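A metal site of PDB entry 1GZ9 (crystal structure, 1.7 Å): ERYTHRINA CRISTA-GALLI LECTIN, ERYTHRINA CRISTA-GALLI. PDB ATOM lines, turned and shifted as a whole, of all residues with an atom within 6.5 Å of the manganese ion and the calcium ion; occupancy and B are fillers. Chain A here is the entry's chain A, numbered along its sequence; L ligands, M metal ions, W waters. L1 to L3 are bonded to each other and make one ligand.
The side-chain amide nitrogen of Asn 133 is in hydrogen-bond range of an oxygen (O1) of LG3 L3 (2.7 Å).
The side-chain carboxylate of Asp 89 is in hydrogen-bond range of an oxygen (O3) of LG2 L2 (2.6 Å).
The backbone NH of Gly 107 is in hydrogen-bond range of an oxygen (O2) of LG2 L2, at 3.0 Å.
An oxygen (O3) of LG3 L3 lies within hydrogen-bond range of the side-chain hydroxyl (OH) of Tyr 108, 3.0 Å away.
The side-chain carboxylate of Glu 127 sits close to the side-chain carboxylate of Asp 146 (2.7 Å).
The backbone carbonyl oxygen (O) of Gly 144 sits at hydrogen-bond distance from the backbone NH (N) of Glu 127 (2.9 Å).
The nearest printed residue that does not touch the manganese ion is Ser 152 (4.2 Å).
Four residues have an atom within 4 Å of the calcium ion: Asp 129, Phe 131, Asn 133 and Asp 136.
OD1 of Asp 136 binds the manganese ion (2.1 Å).
The manganese ion is bound by OD2 of Asp 129 (2.2 Å).
The manganese ion is bound by OE2 of Glu 127 (2.2 Å).
The manganese ion is bound by water W2 (2.2 Å).
NE2 of His 142 is bound to the manganese ion (2.3 Å).
Water W3 binds the manganese ion (2.3 Å).
The manganese ion has six donor atoms within binding distance.
The calcium ion is bound by water W4 (2.4 Å), OD1 of Asn 133 (2.4 Å), O of Phe 131 (2.4 Å), OD2 of Asp 136 (2.4 Å), water W1 (2.4 Å), OD2 of Asp 129 (2.4 Å) and OD1 of Asp 129 (2.4 Å).
Water W3 lies within hydrogen-bond range of the side-chain carboxylate (OE1) of Glu 127, the backbone carbonyl oxygen (O) of Ile 150 and the indole nitrogen (NE1) of Trp 135.
Water W1 lies within hydrogen-bond range of the backbone carbonyl oxygen of Gly 107 and the indole nitrogen of Trp 135.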
ATOM      1  N   ASP A  89      -2.723 -27.322  -4.686  1.00  0.00           N
ATOM      2  CA  ASP A  89      -3.325 -26.067  -5.158  1.00  0.00           C
ATOM      3  C   ASP A  89      -2.620 -25.507  -6.428  1.00  0.00           C
ATOM      4  O   ASP A  89      -3.244 -24.767  -7.199  1.00  0.00           O
ATOM      5  CB  ASP A  89      -3.248 -25.018  -4.055  1.00  0.00           C
ATOM      6  CG  ASP A  89      -4.530 -24.928  -3.216  1.00  0.00           C
ATOM      7  OD1 ASP A  89      -5.557 -24.407  -3.722  1.00  0.00           O
ATOM      8  OD2 ASP A  89      -4.508 -25.385  -2.040  1.00  0.00           O
ATOM      9  N   GLY A 107      -4.691 -21.944  -1.819  1.00  0.00           N
ATOM     10  CA  GLY A 107      -4.946 -21.262  -3.078  1.00  0.00           C
ATOM     11  C   GLY A 107      -4.173 -19.947  -3.263  1.00  0.00           C
ATOM     12  O   GLY A 107      -4.173 -19.373  -4.374  1.00  0.00           O
ATOM     13  N   TYR A 108      -3.507 -19.469  -2.225  1.00  0.00           N
ATOM     14  CA  TYR A 108      -2.743 -18.228  -2.341  1.00  0.00           C
ATOM     15  C   TYR A 108      -1.323 -18.496  -2.823  1.00  0.00           C
ATOM     16  O   TYR A 108      -0.534 -17.554  -3.043  1.00  0.00           O
ATOM     17  CB  TYR A 108      -2.733 -17.478  -1.012  1.00  0.00           C
ATOM     18  CG  TYR A 108      -4.151 -17.232  -0.525  1.00  0.00           C
ATOM     19  CD1 TYR A 108      -4.951 -16.253  -1.101  1.00  0.00           C
ATOM     20  CD2 TYR A 108      -4.720 -18.051   0.478  1.00  0.00           C
ATOM     21  CE1 TYR A 108      -6.284 -16.073  -0.706  1.00  0.00           C
ATOM     22  CE2 TYR A 108      -6.055 -17.879   0.878  1.00  0.00           C
ATOM     23  CZ  TYR A 108      -6.819 -16.889   0.275  1.00  0.00           C
ATOM     24  OH  TYR A 108      -8.152 -16.756   0.620  1.00  0.00           O
ATOM     25  N   LEU A 109      -1.038 -19.778  -2.987  1.00  0.00           N
ATOM     26  CA  LEU A 109       0.201 -20.305  -3.544  1.00  0.00           C
ATOM     27  C   LEU A 109       1.523 -19.870  -2.911  1.00  0.00           C
ATOM     28  O   LEU A 109       2.581 -19.974  -3.557  1.00  0.00           O
ATOM     29  CB  LEU A 109       0.197 -19.998  -5.070  1.00  0.00           C
ATOM     30  CG  LEU A 109      -1.074 -20.431  -5.846  1.00  0.00           C
ATOM     31  CD1 LEU A 109      -0.939 -20.103  -7.380  1.00  0.00           C
ATOM     32  CD2 LEU A 109      -1.230 -21.950  -5.727  1.00  0.00           C
ATOM     33  N   GLU A 127       0.977 -18.310 -12.723  1.00  0.00           N
ATOM     34  CA  GLU A 127       0.525 -19.501 -11.993  1.00  0.00           C
ATOM     35  C   GLU A 127       0.079 -20.646 -12.877  1.00  0.00           C
ATOM     36  O   GLU A 127      -0.286 -20.424 -14.027  1.00  0.00           O
ATOM     37  CB  GLU A 127      -0.629 -19.099 -11.085  1.00  0.00           C
ATOM     38  CG  GLU A 127      -1.882 -18.621 -11.843  1.00  0.00           C
ATOM     39  CD  GLU A 127      -3.113 -18.456 -10.957  1.00  0.00           C
ATOM     40  OE1 GLU A 127      -3.037 -17.802  -9.871  1.00  0.00           O
ATOM     41  OE2 GLU A 127      -4.146 -18.980 -11.406  1.00  0.00           O
ATOM     42  N   ASP A 129      -2.397 -23.253 -11.898  1.00  0.00           N
ATOM     43  CA  ASP A 129      -3.366 -23.457 -10.793  1.00  0.00           C
ATOM     44  C   ASP A 129      -4.222 -24.673 -10.995  1.00  0.00           C
ATOM     45  O   ASP A 129      -4.863 -24.815 -12.040  1.00  0.00           O
ATOM     46  CB  ASP A 129      -4.219 -22.161 -10.755  1.00  0.00           C
ATOM     47  CG  ASP A 129      -5.159 -22.072  -9.561  1.00  0.00           C
ATOM     48  OD1 ASP A 129      -5.330 -23.065  -8.856  1.00  0.00           O
ATOM     49  OD2 ASP A 129      -5.729 -20.973  -9.372  1.00  0.00           O
ATOM     50  N   THR A 130      -4.255 -25.547  -9.985  1.00  0.00           N
ATOM     51  CA  THR A 130      -4.955 -26.807 -10.073  1.00  0.00           C
ATOM     52  C   THR A 130      -6.265 -26.929  -9.315  1.00  0.00           C
ATOM     53  O   THR A 130      -6.919 -27.955  -9.430  1.00  0.00           O
ATOM     54  CB  THR A 130      -4.053 -27.958  -9.580  1.00  0.00           C
ATOM     55  OG1 THR A 130      -3.574 -27.622  -8.279  1.00  0.00           O
ATOM     56  CG2 THR A 130      -2.852 -28.136 -10.492  1.00  0.00           C
ATOM     57  N   PHE A 131      -6.666 -25.884  -8.569  1.00  0.00           N
ATOM     58  CA  PHE A 131      -7.918 -25.972  -7.784  1.00  0.00           C
ATOM     59  C   PHE A 131      -8.704 -24.712  -7.992  1.00  0.00           C
ATOM     60  O   PHE A 131      -8.164 -23.611  -7.798  1.00  0.00           O
ATOM     61  CB  PHE A 131      -7.586 -26.120  -6.292  1.00  0.00           C
ATOM     62  CG  PHE A 131      -8.837 -26.186  -5.406  1.00  0.00           C
ATOM     63  CD1 PHE A 131      -9.427 -27.399  -5.106  1.00  0.00           C
ATOM     64  CD2 PHE A 131      -9.407 -25.002  -4.921  1.00  0.00           C
ATOM     65  CE1 PHE A 131     -10.608 -27.447  -4.318  1.00  0.00           C
ATOM     66  CE2 PHE A 131     -10.586 -25.042  -4.139  1.00  0.00           C
ATOM     67  CZ  PHE A 131     -11.185 -26.256  -3.843  1.00  0.00           C
ATOM     68  N   SER A 132      -9.993 -24.851  -8.303  1.00  0.00           N
ATOM     69  CA  SER A 132     -10.831 -23.657  -8.582  1.00  0.00           C
ATOM     70  C   SER A 132     -11.375 -23.037  -7.282  1.00  0.00           C
ATOM     71  O   SER A 132     -12.358 -23.539  -6.691  1.00  0.00           O
ATOM     72  CB  SER A 132     -12.017 -24.029  -9.480  1.00  0.00           C
ATOM     73  OG  SER A 132     -12.698 -22.862  -9.920  1.00  0.00           O
ATOM     74  N   ASN A 133     -10.711 -21.984  -6.846  1.00  0.00           N
ATOM     75  CA  ASN A 133     -11.121 -21.228  -5.637  1.00  0.00           C
ATOM     76  C   ASN A 133     -12.286 -20.270  -6.009  1.00  0.00           C
ATOM     77  O   ASN A 133     -12.608 -20.094  -7.179  1.00  0.00           O
ATOM     78  CB  ASN A 133      -9.935 -20.391  -5.147  1.00  0.00           C
ATOM     79  CG  ASN A 133      -8.836 -21.258  -4.573  1.00  0.00           C
ATOM     80  OD1 ASN A 133      -7.917 -21.692  -5.282  1.00  0.00           O
ATOM     81  ND2 ASN A 133      -8.946 -21.568  -3.270  1.00  0.00           N
ATOM     82  N   TRP A 135     -12.400 -17.210  -6.471  1.00  0.00           N
ATOM     83  CA  TRP A 135     -11.983 -16.133  -7.352  1.00  0.00           C
ATOM     84  C   TRP A 135     -11.450 -16.656  -8.693  1.00  0.00           C
ATOM     85  O   TRP A 135     -11.013 -15.847  -9.547  1.00  0.00           O
ATOM     86  CB  TRP A 135     -10.838 -15.326  -6.704  1.00  0.00           C
ATOM     87  CG  TRP A 135      -9.638 -16.239  -6.330  1.00  0.00           C
ATOM     88  CD1 TRP A 135      -8.649 -16.710  -7.180  1.00  0.00           C
ATOM     89  CD2 TRP A 135      -9.356 -16.793  -5.041  1.00  0.00           C
ATOM     90  NE1 TRP A 135      -7.770 -17.532  -6.488  1.00  0.00           N
ATOM     91  CE2 TRP A 135      -8.180 -17.590  -5.173  1.00  0.00           C
ATOM     92  CE3 TRP A 135      -9.977 -16.695  -3.780  1.00  0.00           C
ATOM     93  CZ2 TRP A 135      -7.628 -18.279  -4.084  1.00  0.00           C
ATOM     94  CZ3 TRP A 135      -9.428 -17.383  -2.708  1.00  0.00           C
ATOM     95  CH2 TRP A 135      -8.238 -18.167  -2.871  1.00  0.00           C
ATOM     96  N   ASP A 136     -11.465 -17.978  -8.857  1.00  0.00           N
ATOM     97  CA  ASP A 136     -10.927 -18.613 -10.075  1.00  0.00           C
ATOM     98  C   ASP A 136     -11.919 -18.950 -11.161  1.00  0.00           C
ATOM     99  O   ASP A 136     -13.104 -19.057 -10.913  1.00  0.00           O
ATOM    100  CB  ASP A 136     -10.309 -20.000  -9.734  1.00  0.00           C
ATOM    101  CG  ASP A 136      -8.893 -19.908  -9.165  1.00  0.00           C
ATOM    102  OD1 ASP A 136      -8.096 -19.143  -9.704  1.00  0.00           O
ATOM    103  OD2 ASP A 136      -8.598 -20.623  -8.189  1.00  0.00           O
ATOM    104  N   PRO A 137     -11.427 -19.148 -12.400  1.00  0.00           N
ATOM    105  CA  PRO A 137     -12.301 -19.535 -13.494  1.00  0.00           C
ATOM    106  C   PRO A 137     -12.567 -20.986 -13.127  1.00  0.00           C
ATOM    107  O   PRO A 137     -11.818 -21.586 -12.340  1.00  0.00           O
ATOM    108  CB  PRO A 137     -11.404 -19.435 -14.726  1.00  0.00           C
ATOM    109  CG  PRO A 137     -10.013 -19.591 -14.163  1.00  0.00           C
ATOM    110  CD  PRO A 137     -10.096 -18.756 -12.910  1.00  0.00           C
ATOM    111  N   VAL A 140      -9.839 -26.219 -14.428  1.00  0.00           N
ATOM    112  CA  VAL A 140      -8.531 -26.420 -13.843  1.00  0.00           C
ATOM    113  C   VAL A 140      -7.973 -27.685 -14.446  1.00  0.00           C
ATOM    114  O   VAL A 140      -8.706 -28.618 -14.779  1.00  0.00           O
ATOM    115  CB  VAL A 140      -8.542 -26.574 -12.262  1.00  0.00           C
ATOM    116  CG1 VAL A 140      -8.687 -25.186 -11.619  1.00  0.00           C
ATOM    117  CG2 VAL A 140      -9.712 -27.528 -11.812  1.00  0.00           C
ATOM    118  N   HIS A 142      -5.328 -24.298 -14.876  1.00  0.00           N
ATOM    119  CA  HIS A 142      -5.260 -23.153 -15.775  1.00  0.00           C
ATOM    120  C   HIS A 142      -3.945 -22.386 -15.547  1.00  0.00           C
ATOM    121  O   HIS A 142      -3.336 -22.430 -14.476  1.00  0.00           O
ATOM    122  CB  HIS A 142      -6.483 -22.187 -15.622  1.00  0.00           C
ATOM    123  CG  HIS A 142      -6.696 -21.659 -14.238  1.00  0.00           C
ATOM    124  ND1 HIS A 142      -7.625 -22.213 -13.377  1.00  0.00           N
ATOM    125  CD2 HIS A 142      -6.134 -20.636 -13.570  1.00  0.00           C
ATOM    126  CE1 HIS A 142      -7.613 -21.557 -12.234  1.00  0.00           C
ATOM    127  NE2 HIS A 142      -6.718 -20.586 -12.317  1.00  0.00           N
ATOM    128  N   ILE A 143      -3.473 -21.706 -16.594  1.00  0.00           N
ATOM    129  CA  ILE A 143      -2.321 -20.852 -16.419  1.00  0.00           C
ATOM    130  C   ILE A 143      -3.006 -19.521 -16.103  1.00  0.00           C
ATOM    131  O   ILE A 143      -4.086 -19.244 -16.651  1.00  0.00           O
ATOM    132  CB  ILE A 143      -1.596 -20.611 -17.753  1.00  0.00           C
ATOM    133  CG1 ILE A 143      -1.221 -21.957 -18.372  1.00  0.00           C
ATOM    134  CG2 ILE A 143      -0.375 -19.729 -17.523  1.00  0.00           C
ATOM    135  CD1 ILE A 143      -0.486 -21.799 -19.734  1.00  0.00           C
ATOM    136  N   GLY A 144      -2.377 -18.745 -15.245  1.00  0.00           N
ATOM    137  CA  GLY A 144      -2.883 -17.405 -14.945  1.00  0.00           C
ATOM    138  C   GLY A 144      -1.760 -16.361 -14.857  1.00  0.00           C
ATOM    139  O   GLY A 144      -0.625 -16.662 -14.470  1.00  0.00           O
ATOM    140  N   ASP A 146      -0.992 -13.062 -12.927  1.00  0.00           N
ATOM    141  CA  ASP A 146      -1.369 -12.404 -11.675  1.00  0.00           C
ATOM    142  C   ASP A 146      -0.586 -11.134 -11.465  1.00  0.00           C
ATOM    143  O   ASP A 146       0.641 -11.148 -11.438  1.00  0.00           O
ATOM    144  CB  ASP A 146      -1.104 -13.344 -10.464  1.00  0.00           C
ATOM    145  CG  ASP A 146      -1.831 -14.668 -10.562  1.00  0.00           C
ATOM    146  OD1 ASP A 146      -2.668 -14.810 -11.494  1.00  0.00           O
ATOM    147  OD2 ASP A 146      -1.573 -15.581  -9.700  1.00  0.00           O
ATOM    148  N   ILE A 150      -4.109 -12.570  -6.486  1.00  0.00           N
ATOM    149  CA  ILE A 150      -4.256 -13.992  -6.820  1.00  0.00           C
ATOM    150  C   ILE A 150      -5.421 -14.128  -7.852  1.00  0.00           C
ATOM    151  O   ILE A 150      -5.606 -15.184  -8.482  1.00  0.00           O
ATOM    152  CB  ILE A 150      -4.606 -14.828  -5.548  1.00  0.00           C
ATOM    153  CG1 ILE A 150      -4.505 -16.335  -5.861  1.00  0.00           C
ATOM    154  CG2 ILE A 150      -6.003 -14.503  -5.067  1.00  0.00           C
ATOM    155  CD1 ILE A 150      -3.085 -16.781  -6.228  1.00  0.00           C
ATOM    156  N   ARG A 151      -6.204 -13.060  -8.034  1.00  0.00           N
ATOM    157  CA  ARG A 151      -7.311 -13.077  -9.006  1.00  0.00           C
ATOM    158  C   ARG A 151      -6.707 -12.641 -10.318  1.00  0.00           C
ATOM    159  O   ARG A 151      -6.514 -11.424 -10.561  1.00  0.00           O
ATOM    160  CB  ARG A 151      -8.413 -12.092  -8.609  1.00  0.00           C
ATOM    161  CG  ARG A 151      -8.996 -12.432  -7.243  1.00  0.00           C
ATOM    162  CD  ARG A 151     -10.294 -11.656  -6.958  1.00  0.00           C
ATOM    163  NE  ARG A 151     -10.739 -11.924  -5.600  1.00  0.00           N
ATOM    164  CZ  ARG A 151     -11.969 -12.298  -5.268  1.00  0.00           C
ATOM    165  NH1 ARG A 151     -12.897 -12.441  -6.204  1.00  0.00           N
ATOM    166  NH2 ARG A 151     -12.238 -12.602  -3.992  1.00  0.00           N
ATOM    167  N   SER A 152      -6.445 -13.622 -11.197  1.00  0.00           N
ATOM    168  CA  SER A 152      -5.752 -13.351 -12.459  1.00  0.00           C
ATOM    169  C   SER A 152      -6.405 -12.350 -13.390  1.00  0.00           C
ATOM    170  O   SER A 152      -7.633 -12.369 -13.536  1.00  0.00           O
ATOM    171  CB  SER A 152      -5.607 -14.647 -13.251  1.00  0.00           C
ATOM    172  OG  SER A 152      -4.958 -15.630 -12.470  1.00  0.00           O
ATOM    173  N   THR A 155      -6.543 -15.833 -17.821  1.00  0.00           N
ATOM    174  CA  THR A 155      -6.231 -17.249 -17.608  1.00  0.00           C
ATOM    175  C   THR A 155      -6.407 -18.037 -18.888  1.00  0.00           C
ATOM    176  O   THR A 155      -7.072 -17.601 -19.835  1.00  0.00           O
ATOM    177  CB  THR A 155      -7.131 -17.904 -16.498  1.00  0.00           C
ATOM    178  OG1 THR A 155      -8.512 -17.754 -16.858  1.00  0.00           O
ATOM    179  CG2 THR A 155      -6.924 -17.208 -15.150  1.00  0.00           C
HETATM  180  C1  LIG L   1     -12.100 -27.186   4.050  1.00  0.00           C
HETATM  181  C2  LIG L   1     -10.862 -26.649   3.285  1.00  0.00           C
HETATM  182  C3  LIG L   1     -11.248 -25.413   2.451  1.00  0.00           C
HETATM  183  C4  LIG L   1     -11.906 -24.326   3.320  1.00  0.00           C
HETATM  184  C5  LIG L   1     -12.500 -23.193   2.485  1.00  0.00           C
HETATM  185  C6  LIG L   1     -12.645 -26.041   4.922  1.00  0.00           C
HETATM  186  O1  LIG L   1     -13.765 -26.505   5.607  1.00  0.00           O
HETATM  187  O2  LIG L   1     -11.685 -28.295   4.845  1.00  0.00           O
HETATM  188  O3  LIG L   1     -10.350 -27.683   2.476  1.00  0.00           O
HETATM  189  O4  LIG L   1     -10.031 -24.764   1.858  1.00  0.00           O
HETATM  190  O5  LIG L   1     -13.033 -24.919   4.048  1.00  0.00           O
HETATM  191  O6  LIG L   1     -12.604 -21.997   3.283  1.00  0.00           O
HETATM  192  C1  LG2 L   2      -9.724 -25.018   0.447  1.00  0.00           C
HETATM  193  C2  LG2 L   2      -8.683 -24.024   0.095  1.00  0.00           C
HETATM  194  C3  LG2 L   2      -8.337 -24.351  -1.447  1.00  0.00           C
HETATM  195  C4  LG2 L   2      -7.829 -25.802  -1.554  1.00  0.00           C
HETATM  196  C5  LG2 L   2      -8.975 -26.711  -1.036  1.00  0.00           C
HETATM  197  C6  LG2 L   2      -8.620 -28.157  -1.048  1.00  0.00           C
HETATM  198  O1  LG2 L   2      -9.326 -22.748   0.222  1.00  0.00           O
HETATM  199  O2  LG2 L   2      -7.298 -23.424  -1.878  1.00  0.00           O
HETATM  200  O3  LG2 L   2      -6.678 -26.039  -0.740  1.00  0.00           O
HETATM  201  O4  LG2 L   2      -9.278 -26.366   0.331  1.00  0.00           O
HETATM  202  O5  LG2 L   2      -9.815 -28.863  -0.671  1.00  0.00           O
HETATM  203  C1  LG3 L   3      -8.656 -21.501   0.197  1.00  0.00           C
HETATM  204  C2  LG3 L   3      -9.796 -20.466   0.029  1.00  0.00           C
HETATM  205  C3  LG3 L   3     -10.707 -20.198   1.273  1.00  0.00           C
HETATM  206  C4  LG3 L   3      -9.851 -20.089   2.581  1.00  0.00           C
HETATM  207  C5  LG3 L   3      -8.910 -21.324   2.702  1.00  0.00           C
HETATM  208  C6  LG3 L   3      -8.004 -21.268   4.000  1.00  0.00           C
HETATM  209  O1  LG3 L   3     -10.415 -20.559  -1.275  1.00  0.00           O
HETATM  210  O2  LG3 L   3     -11.400 -18.972   1.054  1.00  0.00           O
HETATM  211  O3  LG3 L   3      -9.069 -18.908   2.542  1.00  0.00           O
HETATM  212  O4  LG3 L   3      -7.966 -21.419   1.501  1.00  0.00           O
HETATM  213 MN    MN M   1      -6.159 -19.199 -10.557  1.00  0.00          MN
HETATM  214 CA    CA M   2      -6.707 -21.790  -7.320  1.00  0.00          CA
HETATM  215  O   HOH W   1      -5.566 -19.750  -6.743  1.00  0.00           O
HETATM  216  O   HOH W   2      -6.838 -17.395 -11.632  1.00  0.00           O
HETATM  217  O   HOH W   3      -5.359 -17.914  -8.782  1.00  0.00           O
HETATM  218  O   HOH W   4      -5.318 -23.241  -6.057  1.00  0.00           O
